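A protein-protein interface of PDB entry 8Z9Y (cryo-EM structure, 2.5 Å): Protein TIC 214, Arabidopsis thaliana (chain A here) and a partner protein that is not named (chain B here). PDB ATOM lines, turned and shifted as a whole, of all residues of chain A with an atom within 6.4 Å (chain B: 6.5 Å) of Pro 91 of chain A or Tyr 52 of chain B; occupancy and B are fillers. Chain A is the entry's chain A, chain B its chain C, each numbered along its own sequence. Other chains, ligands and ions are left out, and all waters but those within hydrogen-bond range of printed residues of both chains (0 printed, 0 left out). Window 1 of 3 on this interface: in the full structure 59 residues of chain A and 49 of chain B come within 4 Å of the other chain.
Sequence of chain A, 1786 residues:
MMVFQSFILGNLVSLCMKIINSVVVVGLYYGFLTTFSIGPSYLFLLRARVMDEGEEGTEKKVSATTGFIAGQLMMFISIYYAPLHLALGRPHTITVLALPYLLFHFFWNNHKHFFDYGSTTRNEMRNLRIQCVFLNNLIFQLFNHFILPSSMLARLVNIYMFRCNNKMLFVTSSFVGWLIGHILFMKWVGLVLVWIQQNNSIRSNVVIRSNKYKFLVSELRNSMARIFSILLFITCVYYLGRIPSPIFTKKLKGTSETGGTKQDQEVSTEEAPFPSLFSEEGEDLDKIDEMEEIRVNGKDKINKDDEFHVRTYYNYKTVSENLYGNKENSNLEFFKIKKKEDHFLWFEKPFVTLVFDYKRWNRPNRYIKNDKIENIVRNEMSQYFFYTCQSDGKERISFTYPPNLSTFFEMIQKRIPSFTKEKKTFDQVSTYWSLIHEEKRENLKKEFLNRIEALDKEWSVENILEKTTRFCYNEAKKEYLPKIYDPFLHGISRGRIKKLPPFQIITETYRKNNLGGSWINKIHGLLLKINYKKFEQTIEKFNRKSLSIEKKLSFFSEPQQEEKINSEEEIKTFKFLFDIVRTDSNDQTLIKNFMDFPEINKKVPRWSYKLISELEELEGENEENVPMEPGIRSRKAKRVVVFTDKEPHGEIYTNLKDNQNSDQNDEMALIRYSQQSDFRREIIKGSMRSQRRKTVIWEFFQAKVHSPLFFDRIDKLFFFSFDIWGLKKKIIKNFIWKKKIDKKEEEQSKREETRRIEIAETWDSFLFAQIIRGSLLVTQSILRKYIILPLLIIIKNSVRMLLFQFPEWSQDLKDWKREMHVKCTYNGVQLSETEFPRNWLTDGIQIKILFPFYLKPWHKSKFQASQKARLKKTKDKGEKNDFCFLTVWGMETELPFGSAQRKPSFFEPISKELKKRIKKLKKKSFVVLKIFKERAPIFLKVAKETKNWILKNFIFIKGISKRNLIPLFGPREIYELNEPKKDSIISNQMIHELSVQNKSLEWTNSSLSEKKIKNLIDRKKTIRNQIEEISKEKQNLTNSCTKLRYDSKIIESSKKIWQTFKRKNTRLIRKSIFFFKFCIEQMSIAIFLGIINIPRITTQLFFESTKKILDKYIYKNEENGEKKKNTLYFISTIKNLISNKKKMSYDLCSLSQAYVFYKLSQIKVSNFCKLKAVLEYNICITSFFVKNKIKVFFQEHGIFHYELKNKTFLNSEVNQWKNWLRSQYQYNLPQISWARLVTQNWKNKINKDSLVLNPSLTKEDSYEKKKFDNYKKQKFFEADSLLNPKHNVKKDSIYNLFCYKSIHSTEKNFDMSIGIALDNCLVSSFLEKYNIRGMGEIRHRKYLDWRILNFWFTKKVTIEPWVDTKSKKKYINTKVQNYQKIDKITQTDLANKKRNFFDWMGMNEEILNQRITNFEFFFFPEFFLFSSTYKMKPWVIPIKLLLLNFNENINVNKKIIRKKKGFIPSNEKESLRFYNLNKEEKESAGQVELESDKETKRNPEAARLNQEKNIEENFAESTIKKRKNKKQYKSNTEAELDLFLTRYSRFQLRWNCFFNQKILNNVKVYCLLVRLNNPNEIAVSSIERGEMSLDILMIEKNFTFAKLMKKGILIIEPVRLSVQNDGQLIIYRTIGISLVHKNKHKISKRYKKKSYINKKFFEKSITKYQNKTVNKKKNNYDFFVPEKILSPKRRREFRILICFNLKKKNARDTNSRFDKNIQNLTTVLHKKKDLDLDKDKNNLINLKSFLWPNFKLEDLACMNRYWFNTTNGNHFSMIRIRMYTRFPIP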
ATOM      1  N   HIS A  85      13.399  33.214  20.215  1.00  0.00           N
ATOM      2  CA  HIS A  85      14.617  32.497  19.855  1.00  0.00           C
ATOM      3  C   HIS A  85      14.295  31.198  19.130  1.00  0.00           C
ATOM      4  O   HIS A  85      14.947  30.854  18.138  1.00  0.00           O
ATOM      5  CB  HIS A  85      15.455  32.220  21.101  1.00  0.00           C
ATOM      6  CG  HIS A  85      16.741  31.512  20.814  1.00  0.00           C
ATOM      7  ND1 HIS A  85      17.793  32.117  20.161  1.00  0.00           N
ATOM      8  CD2 HIS A  85      17.146  30.250  21.089  1.00  0.00           C
ATOM      9  CE1 HIS A  85      18.791  31.258  20.047  1.00  0.00           C
ATOM     10  NE2 HIS A  85      18.424  30.118  20.602  1.00  0.00           N
ATOM     11  N   LEU A  88      12.962  32.133  15.520  1.00  0.00           N
ATOM     12  CA  LEU A  88      13.952  32.650  14.584  1.00  0.00           C
ATOM     13  C   LEU A  88      15.302  31.951  14.706  1.00  0.00           C
ATOM     14  O   LEU A  88      16.314  32.481  14.237  1.00  0.00           O
ATOM     15  CB  LEU A  88      14.119  34.158  14.774  1.00  0.00           C
ATOM     16  CG  LEU A  88      12.836  34.987  14.723  1.00  0.00           C
ATOM     17  CD1 LEU A  88      13.111  36.425  15.125  1.00  0.00           C
ATOM     18  CD2 LEU A  88      12.213  34.926  13.340  1.00  0.00           C
ATOM     19  N   GLY A  89      15.342  30.775  15.324  1.00  0.00           N
ATOM     20  CA  GLY A  89      16.592  30.062  15.497  1.00  0.00           C
ATOM     21  C   GLY A  89      16.822  28.967  14.476  1.00  0.00           C
ATOM     22  O   GLY A  89      17.642  28.071  14.695  1.00  0.00           O
ATOM     23  N   ARG A  90      16.106  29.026  13.357  1.00  0.00           N
ATOM     24  CA  ARG A  90      16.198  27.993  12.331  1.00  0.00           C
ATOM     25  C   ARG A  90      16.990  28.511  11.141  1.00  0.00           C
ATOM     26  O   ARG A  90      16.477  29.347  10.379  1.00  0.00           O
ATOM     27  CB  ARG A  90      14.802  27.553  11.891  1.00  0.00           C
ATOM     28  CG  ARG A  90      13.972  26.945  13.007  1.00  0.00           C
ATOM     29  CD  ARG A  90      12.533  27.428  12.949  1.00  0.00           C
ATOM     30  NE  ARG A  90      11.830  27.184  14.202  1.00  0.00           N
ATOM     31  CZ  ARG A  90      11.008  26.164  14.414  1.00  0.00           C
ATOM     32  NH1 ARG A  90      10.762  25.268  13.473  1.00  0.00           N
ATOM     33  NH2 ARG A  90      10.421  26.040  15.601  1.00  0.00           N
ATOM     34  N   PRO A  91      18.226  28.059  10.935  1.00  0.00           N
ATOM     35  CA  PRO A  91      19.004  28.529   9.780  1.00  0.00           C
ATOM     36  C   PRO A  91      18.471  28.014   8.454  1.00  0.00           C
ATOM     37  O   PRO A  91      18.329  28.779   7.492  1.00  0.00           O
ATOM     38  CB  PRO A  91      20.410  27.985  10.062  1.00  0.00           C
ATOM     39  CG  PRO A  91      20.201  26.830  10.979  1.00  0.00           C
ATOM     40  CD  PRO A  91      19.004  27.168  11.811  1.00  0.00           C
ATOM     41  N   HIS A  92      18.178  26.713   8.397  1.00  0.00           N
ATOM     42  CA  HIS A  92      17.773  26.091   7.140  1.00  0.00           C
ATOM     43  C   HIS A  92      16.485  26.706   6.610  1.00  0.00           C
ATOM     44  O   HIS A  92      16.383  27.034   5.422  1.00  0.00           O
ATOM     45  CB  HIS A  92      17.608  24.583   7.332  1.00  0.00           C
ATOM     46  CG  HIS A  92      18.784  23.920   7.977  1.00  0.00           C
ATOM     47  ND1 HIS A  92      18.961  23.880   9.343  1.00  0.00           N
ATOM     48  CD2 HIS A  92      19.844  23.269   7.442  1.00  0.00           C
ATOM     49  CE1 HIS A  92      20.079  23.234   9.621  1.00  0.00           C
ATOM     50  NE2 HIS A  92      20.634  22.852   8.485  1.00  0.00           N
ATOM     51  N   THR A  93      15.491  26.879   7.484  1.00  0.00           N
ATOM     52  CA  THR A  93      14.197  27.394   7.050  1.00  0.00           C
ATOM     53  C   THR A  93      14.323  28.810   6.500  1.00  0.00           C
ATOM     54  O   THR A  93      13.805  29.117   5.419  1.00  0.00           O
ATOM     55  CB  THR A  93      13.204  27.357   8.212  1.00  0.00           C
ATOM     56  OG1 THR A  93      12.993  25.999   8.617  1.00  0.00           O
ATOM     57  CG2 THR A  93      11.876  27.968   7.799  1.00  0.00           C
ATOM     58  N   ILE A  94      15.017  29.684   7.230  1.00  0.00           N
ATOM     59  CA  ILE A  94      15.159  31.072   6.799  1.00  0.00           C
ATOM     60  C   ILE A  94      15.952  31.152   5.502  1.00  0.00           C
ATOM     61  O   ILE A  94      15.584  31.887   4.574  1.00  0.00           O
ATOM     62  CB  ILE A  94      15.809  31.910   7.916  1.00  0.00           C
ATOM     63  CG1 ILE A  94      14.817  32.126   9.060  1.00  0.00           C
ATOM     64  CG2 ILE A  94      16.295  33.243   7.375  1.00  0.00           C
ATOM     65  CD1 ILE A  94      15.439  32.728  10.297  1.00  0.00           C
ATOM     66  N   THR A  95      17.051  30.399   5.413  1.00  0.00           N
ATOM     67  CA  THR A  95      17.870  30.433   4.206  1.00  0.00           C
ATOM     68  C   THR A  95      17.094  29.928   2.996  1.00  0.00           C
ATOM     69  O   THR A  95      17.220  30.479   1.896  1.00  0.00           O
ATOM     70  CB  THR A  95      19.145  29.617   4.408  1.00  0.00           C
ATOM     71  OG1 THR A  95      18.827  28.389   5.073  1.00  0.00           O
ATOM     72  CG2 THR A  95      20.145  30.399   5.246  1.00  0.00           C
ATOM     73  N   VAL A  96      16.291  28.877   3.175  1.00  0.00           N
ATOM     74  CA  VAL A  96      15.489  28.364   2.070  1.00  0.00           C
ATOM     75  C   VAL A  96      14.420  29.373   1.668  1.00  0.00           C
ATOM     76  O   VAL A  96      14.194  29.615   0.476  1.00  0.00           O
ATOM     77  CB  VAL A  96      14.880  27.002   2.448  1.00  0.00           C
ATOM     78  CG1 VAL A  96      13.664  26.698   1.588  1.00  0.00           C
ATOM     79  CG2 VAL A  96      15.922  25.904   2.314  1.00  0.00           C
ATOM     80  N   PHE A 143      14.993  38.155   8.038  1.00  0.00           N
ATOM     81  CA  PHE A 143      15.583  37.164   7.148  1.00  0.00           C
ATOM     82  C   PHE A 143      17.096  37.045   7.290  1.00  0.00           C
ATOM     83  O   PHE A 143      17.701  36.232   6.584  1.00  0.00           O
ATOM     84  CB  PHE A 143      15.227  37.487   5.694  1.00  0.00           C
ATOM     85  CG  PHE A 143      13.858  37.026   5.294  1.00  0.00           C
ATOM     86  CD1 PHE A 143      13.426  35.748   5.604  1.00  0.00           C
ATOM     87  CD2 PHE A 143      12.999  37.872   4.613  1.00  0.00           C
ATOM     88  CE1 PHE A 143      12.165  35.320   5.240  1.00  0.00           C
ATOM     89  CE2 PHE A 143      11.737  37.448   4.247  1.00  0.00           C
ATOM     90  CZ  PHE A 143      11.320  36.171   4.561  1.00  0.00           C
ATOM     91  N   ASN A 144      17.713  37.828   8.176  1.00  0.00           N
ATOM     92  CA  ASN A 144      19.154  37.766   8.431  1.00  0.00           C
ATOM     93  C   ASN A 144      19.949  38.011   7.146  1.00  0.00           C
ATOM     94  O   ASN A 144      20.676  37.146   6.651  1.00  0.00           O
ATOM     95  CB  ASN A 144      19.537  36.430   9.077  1.00  0.00           C
ATOM     96  CG  ASN A 144      20.938  36.439   9.650  1.00  0.00           C
ATOM     97  OD1 ASN A 144      21.416  37.463  10.137  1.00  0.00           O
ATOM     98  ND2 ASN A 144      21.605  35.292   9.598  1.00  0.00           N
ATOM     99  N   GLU A 348      12.264  23.111  16.942  1.00  0.00           N
ATOM    100  CA  GLU A 348      13.061  23.293  15.736  1.00  0.00           C
ATOM    101  C   GLU A 348      12.801  22.140  14.778  1.00  0.00           C
ATOM    102  O   GLU A 348      13.146  20.992  15.078  1.00  0.00           O
ATOM    103  CB  GLU A 348      14.551  23.374  16.072  1.00  0.00           C
ATOM    104  CG  GLU A 348      14.903  24.385  17.147  1.00  0.00           C
ATOM    105  CD  GLU A 348      14.872  25.809  16.637  1.00  0.00           C
ATOM    106  OE1 GLU A 348      15.662  26.132  15.726  1.00  0.00           O
ATOM    107  OE2 GLU A 348      14.062  26.606  17.153  1.00  0.00           O
ATOM    108  N   PRO A 350      13.641  21.729  11.043  1.00  0.00           N
ATOM    109  CA  PRO A 350      14.164  21.634   9.674  1.00  0.00           C
ATOM    110  C   PRO A 350      14.323  20.202   9.190  1.00  0.00           C
ATOM    111  O   PRO A 350      14.823  19.992   8.079  1.00  0.00           O
ATOM    112  CB  PRO A 350      15.540  22.323   9.783  1.00  0.00           C
ATOM    113  CG  PRO A 350      15.589  22.933  11.166  1.00  0.00           C
ATOM    114  CD  PRO A 350      14.721  22.050  11.987  1.00  0.00           C
ATOM    115  N   PHE A 356      19.575  19.926   2.151  1.00  0.00           N
ATOM    116  CA  PHE A 356      20.939  20.443   2.182  1.00  0.00           C
ATOM    117  C   PHE A 356      21.962  19.356   1.872  1.00  0.00           C
ATOM    118  O   PHE A 356      22.955  19.619   1.187  1.00  0.00           O
ATOM    119  CB  PHE A 356      21.221  21.094   3.536  1.00  0.00           C
ATOM    120  CG  PHE A 356      20.647  22.477   3.668  1.00  0.00           C
ATOM    121  CD1 PHE A 356      19.283  22.665   3.808  1.00  0.00           C
ATOM    122  CD2 PHE A 356      21.470  23.589   3.637  1.00  0.00           C
ATOM    123  CE1 PHE A 356      18.751  23.934   3.924  1.00  0.00           C
ATOM    124  CE2 PHE A 356      20.944  24.862   3.752  1.00  0.00           C
ATOM    125  CZ  PHE A 356      19.582  25.034   3.895  1.00  0.00           C
ATOM    126  N   ASN B  48      26.332  36.737   6.644  1.00  0.00           N
ATOM    127  CA  ASN B  48      25.087  37.177   7.248  1.00  0.00           C
ATOM    128  C   ASN B  48      25.364  38.035   8.480  1.00  0.00           C
ATOM    129  O   ASN B  48      26.479  38.079   9.006  1.00  0.00           O
ATOM    130  CB  ASN B  48      24.222  35.977   7.627  1.00  0.00           C
ATOM    131  CG  ASN B  48      23.835  35.139   6.429  1.00  0.00           C
ATOM    132  OD1 ASN B  48      23.556  35.666   5.353  1.00  0.00           O
ATOM    133  ND2 ASN B  48      23.820  33.823   6.606  1.00  0.00           N
ATOM    134  N   PHE B  50      24.100  37.707  11.539  1.00  0.00           N
ATOM    135  CA  PHE B  50      24.267  36.894  12.733  1.00  0.00           C
ATOM    136  C   PHE B  50      24.767  35.503  12.373  1.00  0.00           C
ATOM    137  O   PHE B  50      24.558  35.007  11.263  1.00  0.00           O
ATOM    138  CB  PHE B  50      22.954  36.765  13.518  1.00  0.00           C
ATOM    139  CG  PHE B  50      22.549  38.015  14.237  1.00  0.00           C
ATOM    140  CD1 PHE B  50      23.285  38.479  15.313  1.00  0.00           C
ATOM    141  CD2 PHE B  50      21.420  38.716  13.852  1.00  0.00           C
ATOM    142  CE1 PHE B  50      22.913  39.628  15.982  1.00  0.00           C
ATOM    143  CE2 PHE B  50      21.043  39.865  14.518  1.00  0.00           C
ATOM    144  CZ  PHE B  50      21.789  40.322  15.585  1.00  0.00           C
ATOM    145  N   ASN B  51      25.435  34.879  13.337  1.00  0.00           N
ATOM    146  CA  ASN B  51      25.791  33.470  13.276  1.00  0.00           C
ATOM    147  C   ASN B  51      24.866  32.709  14.215  1.00  0.00           C
ATOM    148  O   ASN B  51      24.752  33.056  15.395  1.00  0.00           O
ATOM    149  CB  ASN B  51      27.255  33.249  13.661  1.00  0.00           C
ATOM    150  CG  ASN B  51      27.738  31.847  13.346  1.00  0.00           C
ATOM    151  OD1 ASN B  51      26.959  30.986  12.936  1.00  0.00           O
ATOM    152  ND2 ASN B  51      29.029  31.612  13.535  1.00  0.00           N
ATOM    153  N   TYR B  52      24.203  31.679  13.685  1.00  0.00           N
ATOM    154  CA  TYR B  52      23.168  30.991  14.450  1.00  0.00           C
ATOM    155  C   TYR B  52      23.747  30.297  15.677  1.00  0.00           C
ATOM    156  O   TYR B  52      23.158  30.346  16.766  1.00  0.00           O
ATOM    157  CB  TYR B  52      22.444  29.994  13.549  1.00  0.00           C
ATOM    158  CG  TYR B  52      21.691  30.661  12.422  1.00  0.00           C
ATOM    159  CD1 TYR B  52      20.447  31.239  12.637  1.00  0.00           C
ATOM    160  CD2 TYR B  52      22.235  30.735  11.148  1.00  0.00           C
ATOM    161  CE1 TYR B  52      19.760  31.855  11.610  1.00  0.00           C
ATOM    162  CE2 TYR B  52      21.556  31.348  10.115  1.00  0.00           C
ATOM    163  CZ  TYR B  52      20.319  31.907  10.352  1.00  0.00           C
ATOM    164  OH  TYR B  52      19.640  32.521   9.326  1.00  0.00           O
ATOM    165  N   HIS B  53      24.901  29.645  15.523  1.00  0.00           N
ATOM    166  CA  HIS B  53      25.532  29.002  16.668  1.00  0.00           C
ATOM    167  C   HIS B  53      25.950  30.021  17.718  1.00  0.00           C
ATOM    168  O   HIS B  53      25.895  29.732  18.916  1.00  0.00           O
ATOM    169  CB  HIS B  53      26.736  28.176  16.221  1.00  0.00           C
ATOM    170  CG  HIS B  53      27.298  27.303  17.297  1.00  0.00           C
ATOM    171  ND1 HIS B  53      26.745  26.085  17.630  1.00  0.00           N
ATOM    172  CD2 HIS B  53      28.357  27.474  18.122  1.00  0.00           C
ATOM    173  CE1 HIS B  53      27.443  25.540  18.611  1.00  0.00           C
ATOM    174  NE2 HIS B  53      28.426  26.363  18.929  1.00  0.00           N
ATOM    175  N   ASP B  54      26.366  31.216  17.292  1.00  0.00           N
ATOM    176  CA  ASP B  54      26.690  32.268  18.250  1.00  0.00           C
ATOM    177  C   ASP B  54      25.460  32.685  19.046  1.00  0.00           C
ATOM    178  O   ASP B  54      25.536  32.886  20.264  1.00  0.00           O
ATOM    179  CB  ASP B  54      27.293  33.469  17.525  1.00  0.00           C
ATOM    180  CG  ASP B  54      28.663  33.175  16.952  1.00  0.00           C
ATOM    181  OD1 ASP B  54      29.023  31.984  16.854  1.00  0.00           O
ATOM    182  OD2 ASP B  54      29.381  34.134  16.601  1.00  0.00           O
ATOM    183  N   LYS B  55      24.316  32.825  18.371  1.00  0.00           N
ATOM    184  CA  LYS B  55      23.079  33.153  19.071  1.00  0.00           C
ATOM    185  C   LYS B  55      22.704  32.062  20.065  1.00  0.00           C
ATOM    186  O   LYS B  55      22.303  32.353  21.200  1.00  0.00           O
ATOM    187  CB  LYS B  55      21.950  33.369  18.065  1.00  0.00           C
ATOM    188  CG  LYS B  55      21.742  34.817  17.656  1.00  0.00           C
ATOM    189  CD  LYS B  55      20.342  35.033  17.104  1.00  0.00           C
ATOM    190  CE  LYS B  55      19.283  34.498  18.056  1.00  0.00           C
ATOM    191  NZ  LYS B  55      17.907  34.861  17.620  1.00  0.00           N
ATOM    192  N   TRP B  56      22.828  30.797  19.653  1.00  0.00           N
ATOM    193  CA  TRP B  56      22.520  29.697  20.561  1.00  0.00           C
ATOM    194  C   TRP B  56      23.455  29.696  21.762  1.00  0.00           C
ATOM    195  O   TRP B  56      23.022  29.463  22.897  1.00  0.00           O
ATOM    196  CB  TRP B  56      22.598  28.366  19.817  1.00  0.00           C
ATOM    197  CG  TRP B  56      21.285  27.923  19.260  1.00  0.00           C
ATOM    198  CD1 TRP B  56      20.917  27.900  17.949  1.00  0.00           C
ATOM    199  CD2 TRP B  56      20.159  27.442  20.001  1.00  0.00           C
ATOM    200  NE1 TRP B  56      19.632  27.433  17.825  1.00  0.00           N
ATOM    201  CE2 TRP B  56      19.145  27.144  19.072  1.00  0.00           C
ATOM    202  CE3 TRP B  56      19.911  27.232  21.360  1.00  0.00           C
ATOM    203  CZ2 TRP B  56      17.903  26.649  19.457  1.00  0.00           C
ATOM    204  CZ3 TRP B  56      18.677  26.742  21.741  1.00  0.00           C
ATOM    205  CH2 TRP B  56      17.689  26.455  20.793  1.00  0.00           C
ATOM    206  N   MET B  57      24.745  29.954  21.531  1.00  0.00           N
ATOM    207  CA  MET B  57      25.703  29.998  22.628  1.00  0.00           C
ATOM    208  C   MET B  57      25.383  31.127  23.596  1.00  0.00           C
ATOM    209  O   MET B  57      25.463  30.946  24.815  1.00  0.00           O
ATOM    210  CB  MET B  57      27.121  30.148  22.079  1.00  0.00           C
ATOM    211  CG  MET B  57      28.210  29.922  23.112  1.00  0.00           C
ATOM    212  SD  MET B  57      29.391  28.655  22.611  1.00  0.00           S
ATOM    213  CE  MET B  57      29.795  29.212  20.959  1.00  0.00           C
ATOM    214  N   TRP B  78      19.678  23.287  23.388  1.00  0.00           N
ATOM    215  CA  TRP B  78      20.293  22.861  22.136  1.00  0.00           C
ATOM    216  C   TRP B  78      20.428  21.346  22.067  1.00  0.00           C
ATOM    217  O   TRP B  78      20.338  20.764  20.981  1.00  0.00           O
ATOM    218  CB  TRP B  78      21.658  23.534  21.973  1.00  0.00           C
ATOM    219  CG  TRP B  78      22.511  22.962  20.880  1.00  0.00           C
ATOM    220  CD1 TRP B  78      23.343  21.883  20.965  1.00  0.00           C
ATOM    221  CD2 TRP B  78      22.625  23.449  19.537  1.00  0.00           C
ATOM    222  NE1 TRP B  78      23.961  21.665  19.759  1.00  0.00           N
ATOM    223  CE2 TRP B  78      23.537  22.612  18.866  1.00  0.00           C
ATOM    224  CE3 TRP B  78      22.041  24.508  18.838  1.00  0.00           C
ATOM    225  CZ2 TRP B  78      23.880  22.803  17.530  1.00  0.00           C
ATOM    226  CZ3 TRP B  78      22.383  24.695  17.512  1.00  0.00           C
ATOM    227  CH2 TRP B  78      23.293  23.847  16.872  1.00  0.00           C
ATOM    228  N   VAL B  85      19.904  17.360  12.967  1.00  0.00           N
ATOM    229  CA  VAL B  85      19.921  18.761  12.564  1.00  0.00           C
ATOM    230  C   VAL B  85      21.209  19.357  13.113  1.00  0.00           C
ATOM    231  O   VAL B  85      21.816  20.244  12.501  1.00  0.00           O
ATOM    232  CB  VAL B  85      18.684  19.521  13.075  1.00  0.00           C
ATOM    233  CG1 VAL B  85      18.715  20.966  12.606  1.00  0.00           C
ATOM    234  CG2 VAL B  85      17.410  18.836  12.612  1.00  0.00           C
ATOM    235  N   TYR B  89      24.011  21.030  10.752  1.00  0.00           N
ATOM    236  CA  TYR B  89      24.624  22.337  10.964  1.00  0.00           C
ATOM    237  C   TYR B  89      26.134  22.219  11.112  1.00  0.00           C
ATOM    238  O   TYR B  89      26.881  23.015  10.536  1.00  0.00           O
ATOM    239  CB  TYR B  89      24.022  23.024  12.188  1.00  0.00           C
ATOM    240  CG  TYR B  89      24.483  24.456  12.344  1.00  0.00           C
ATOM    241  CD1 TYR B  89      23.859  25.487  11.656  1.00  0.00           C
ATOM    242  CD2 TYR B  89      25.551  24.776  13.173  1.00  0.00           C
ATOM    243  CE1 TYR B  89      24.282  26.794  11.791  1.00  0.00           C
ATOM    244  CE2 TYR B  89      25.980  26.080  13.315  1.00  0.00           C
ATOM    245  CZ  TYR B  89      25.342  27.085  12.622  1.00  0.00           C
ATOM    246  OH  TYR B  89      25.766  28.387  12.762  1.00  0.00           O
ATOM    247  N   PHE B  97      26.457  28.797   6.205  1.00  0.00           N
ATOM    248  CA  PHE B  97      26.220  29.833   7.211  1.00  0.00           C
ATOM    249  C   PHE B  97      27.544  30.199   7.869  1.00  0.00           C
ATOM    250  O   PHE B  97      27.797  29.844   9.027  1.00  0.00           O
ATOM    251  CB  PHE B  97      25.209  29.361   8.257  1.00  0.00           C
ATOM    252  CG  PHE B  97      24.207  28.376   7.732  1.00  0.00           C
ATOM    253  CD1 PHE B  97      23.236  28.768   6.827  1.00  0.00           C
ATOM    254  CD2 PHE B  97      24.238  27.054   8.142  1.00  0.00           C
ATOM    255  CE1 PHE B  97      22.314  27.859   6.345  1.00  0.00           C
ATOM    256  CE2 PHE B  97      23.320  26.142   7.663  1.00  0.00           C
ATOM    257  CZ  PHE B  97      22.356  26.545   6.764  1.00  0.00           C
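Of the 13 printed residues of chain B, 8 touch a printed residue of chain A.
Printed residues of chain B that touch a printed residue of chain A: Asn 48, Phe 50, Tyr 52, Lys 55, Trp 56, Val 85, Tyr 89 and Phe 97.
Hydrophobic or aromatic side chains of chain B within 4 Å of the printed part of chain A: Phe 50, Tyr 52, Trp 56, Val 85, Tyr 89 and Phe 97.
Among the printed residues, 13 pairs touch across the chains.
The side-chain hydroxyl (OG1) of Thr 95 of chain A lies within hydrogen-bond range of the backbone carbonyl oxygen (O) of Pro 91 of chain A (2.5 Å).
The side-chain hydroxyl (OG1) of Thr 95 of chain A lies within hydrogen-bond range of the backbone carbonyl oxygen (O) of His 92 of chain A, 2.8 Å away.
The side-chain amide oxygen (OD1) of Asn 51 of chain B lies within hydrogen-bond range of the side-chain hydroxyl (OH) of Tyr 89 of chain B (2.9 Å).
The backbone NH (N) of His 53 of chain B is in hydrogen-bond range of the side-chain hydroxyl (OH) of Tyr 89 of chain B, 3.2 Å away.
Printed residues of chain B within 4 Å of His 85 of chain A: Lys 55 (3.5 Å) and Trp 56 (3.2 Å).
Of chain B, only Tyr 52 (3.5 Å) and Tyr 89 (3.96 Å) come within 4 Å of Pro 91 of chain A.
Of the printed residues of chain B, Ile 94 of chain A touches Tyr 52 (3.9 Å).
Printed residues of chain B within 4 Å of Pro 350 of chain A: Val 85.
Printed residues of chain B within 4 Å of Phe 356 of chain A: Phe 97 (3.7 Å).
Of the printed residues of chain A, Asn 48 of chain B touches Asn 144 (3.3 Å).
Tyr 52 of chain B touches just these residues of chain A: Pro 91, Ile 94 and Asn 144.
O of Asn 144 of chain A sits close to OD1 of Asn 48 of chain B, at 3.5 Å.
The side-chain amide oxygen (OD1) of Asn 144 of chain A lies within hydrogen-bond range of the backbone NH (N) of Phe 50 of chain B (3.0 Å).
The side-chain amide nitrogen (ND2) of Asn 144 of chain A lies within hydrogen-bond range of the side-chain hydroxyl (OH) of Tyr 52 of chain B.
His 85 of chain A touches Lys 55 of chain B (ND1 to CE, 3.5 Å).
NE2 of His 85 of chain A touches CD2 of Trp 56 of chain B (3.2 Å).
Trp 56 of chain B touches Gly 89 of chain A (NE1 to O, 3.8 Å).
Pro 91 of chain A touches Tyr 52 of chain B (CB to CD2, 3.5 Å).
Tyr 89 of chain B touches Pro 91 of chain A.
His 92 of chain A touches Val 85 of chain B.
Ile 94 of chain A touches Tyr 52 of chain B (CG2 to OH, 3.9 Å).
Thr 95 of chain A touches Phe 97 of chain B (CG2 to CE1, 3.5 Å).
Pro 350 of chain A touches Val 85 of chain B (CG to CG1, 3.96 Å).
Phe 356 of chain A touches Phe 97 of chain B (CE2 to CZ, 3.7 Å).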
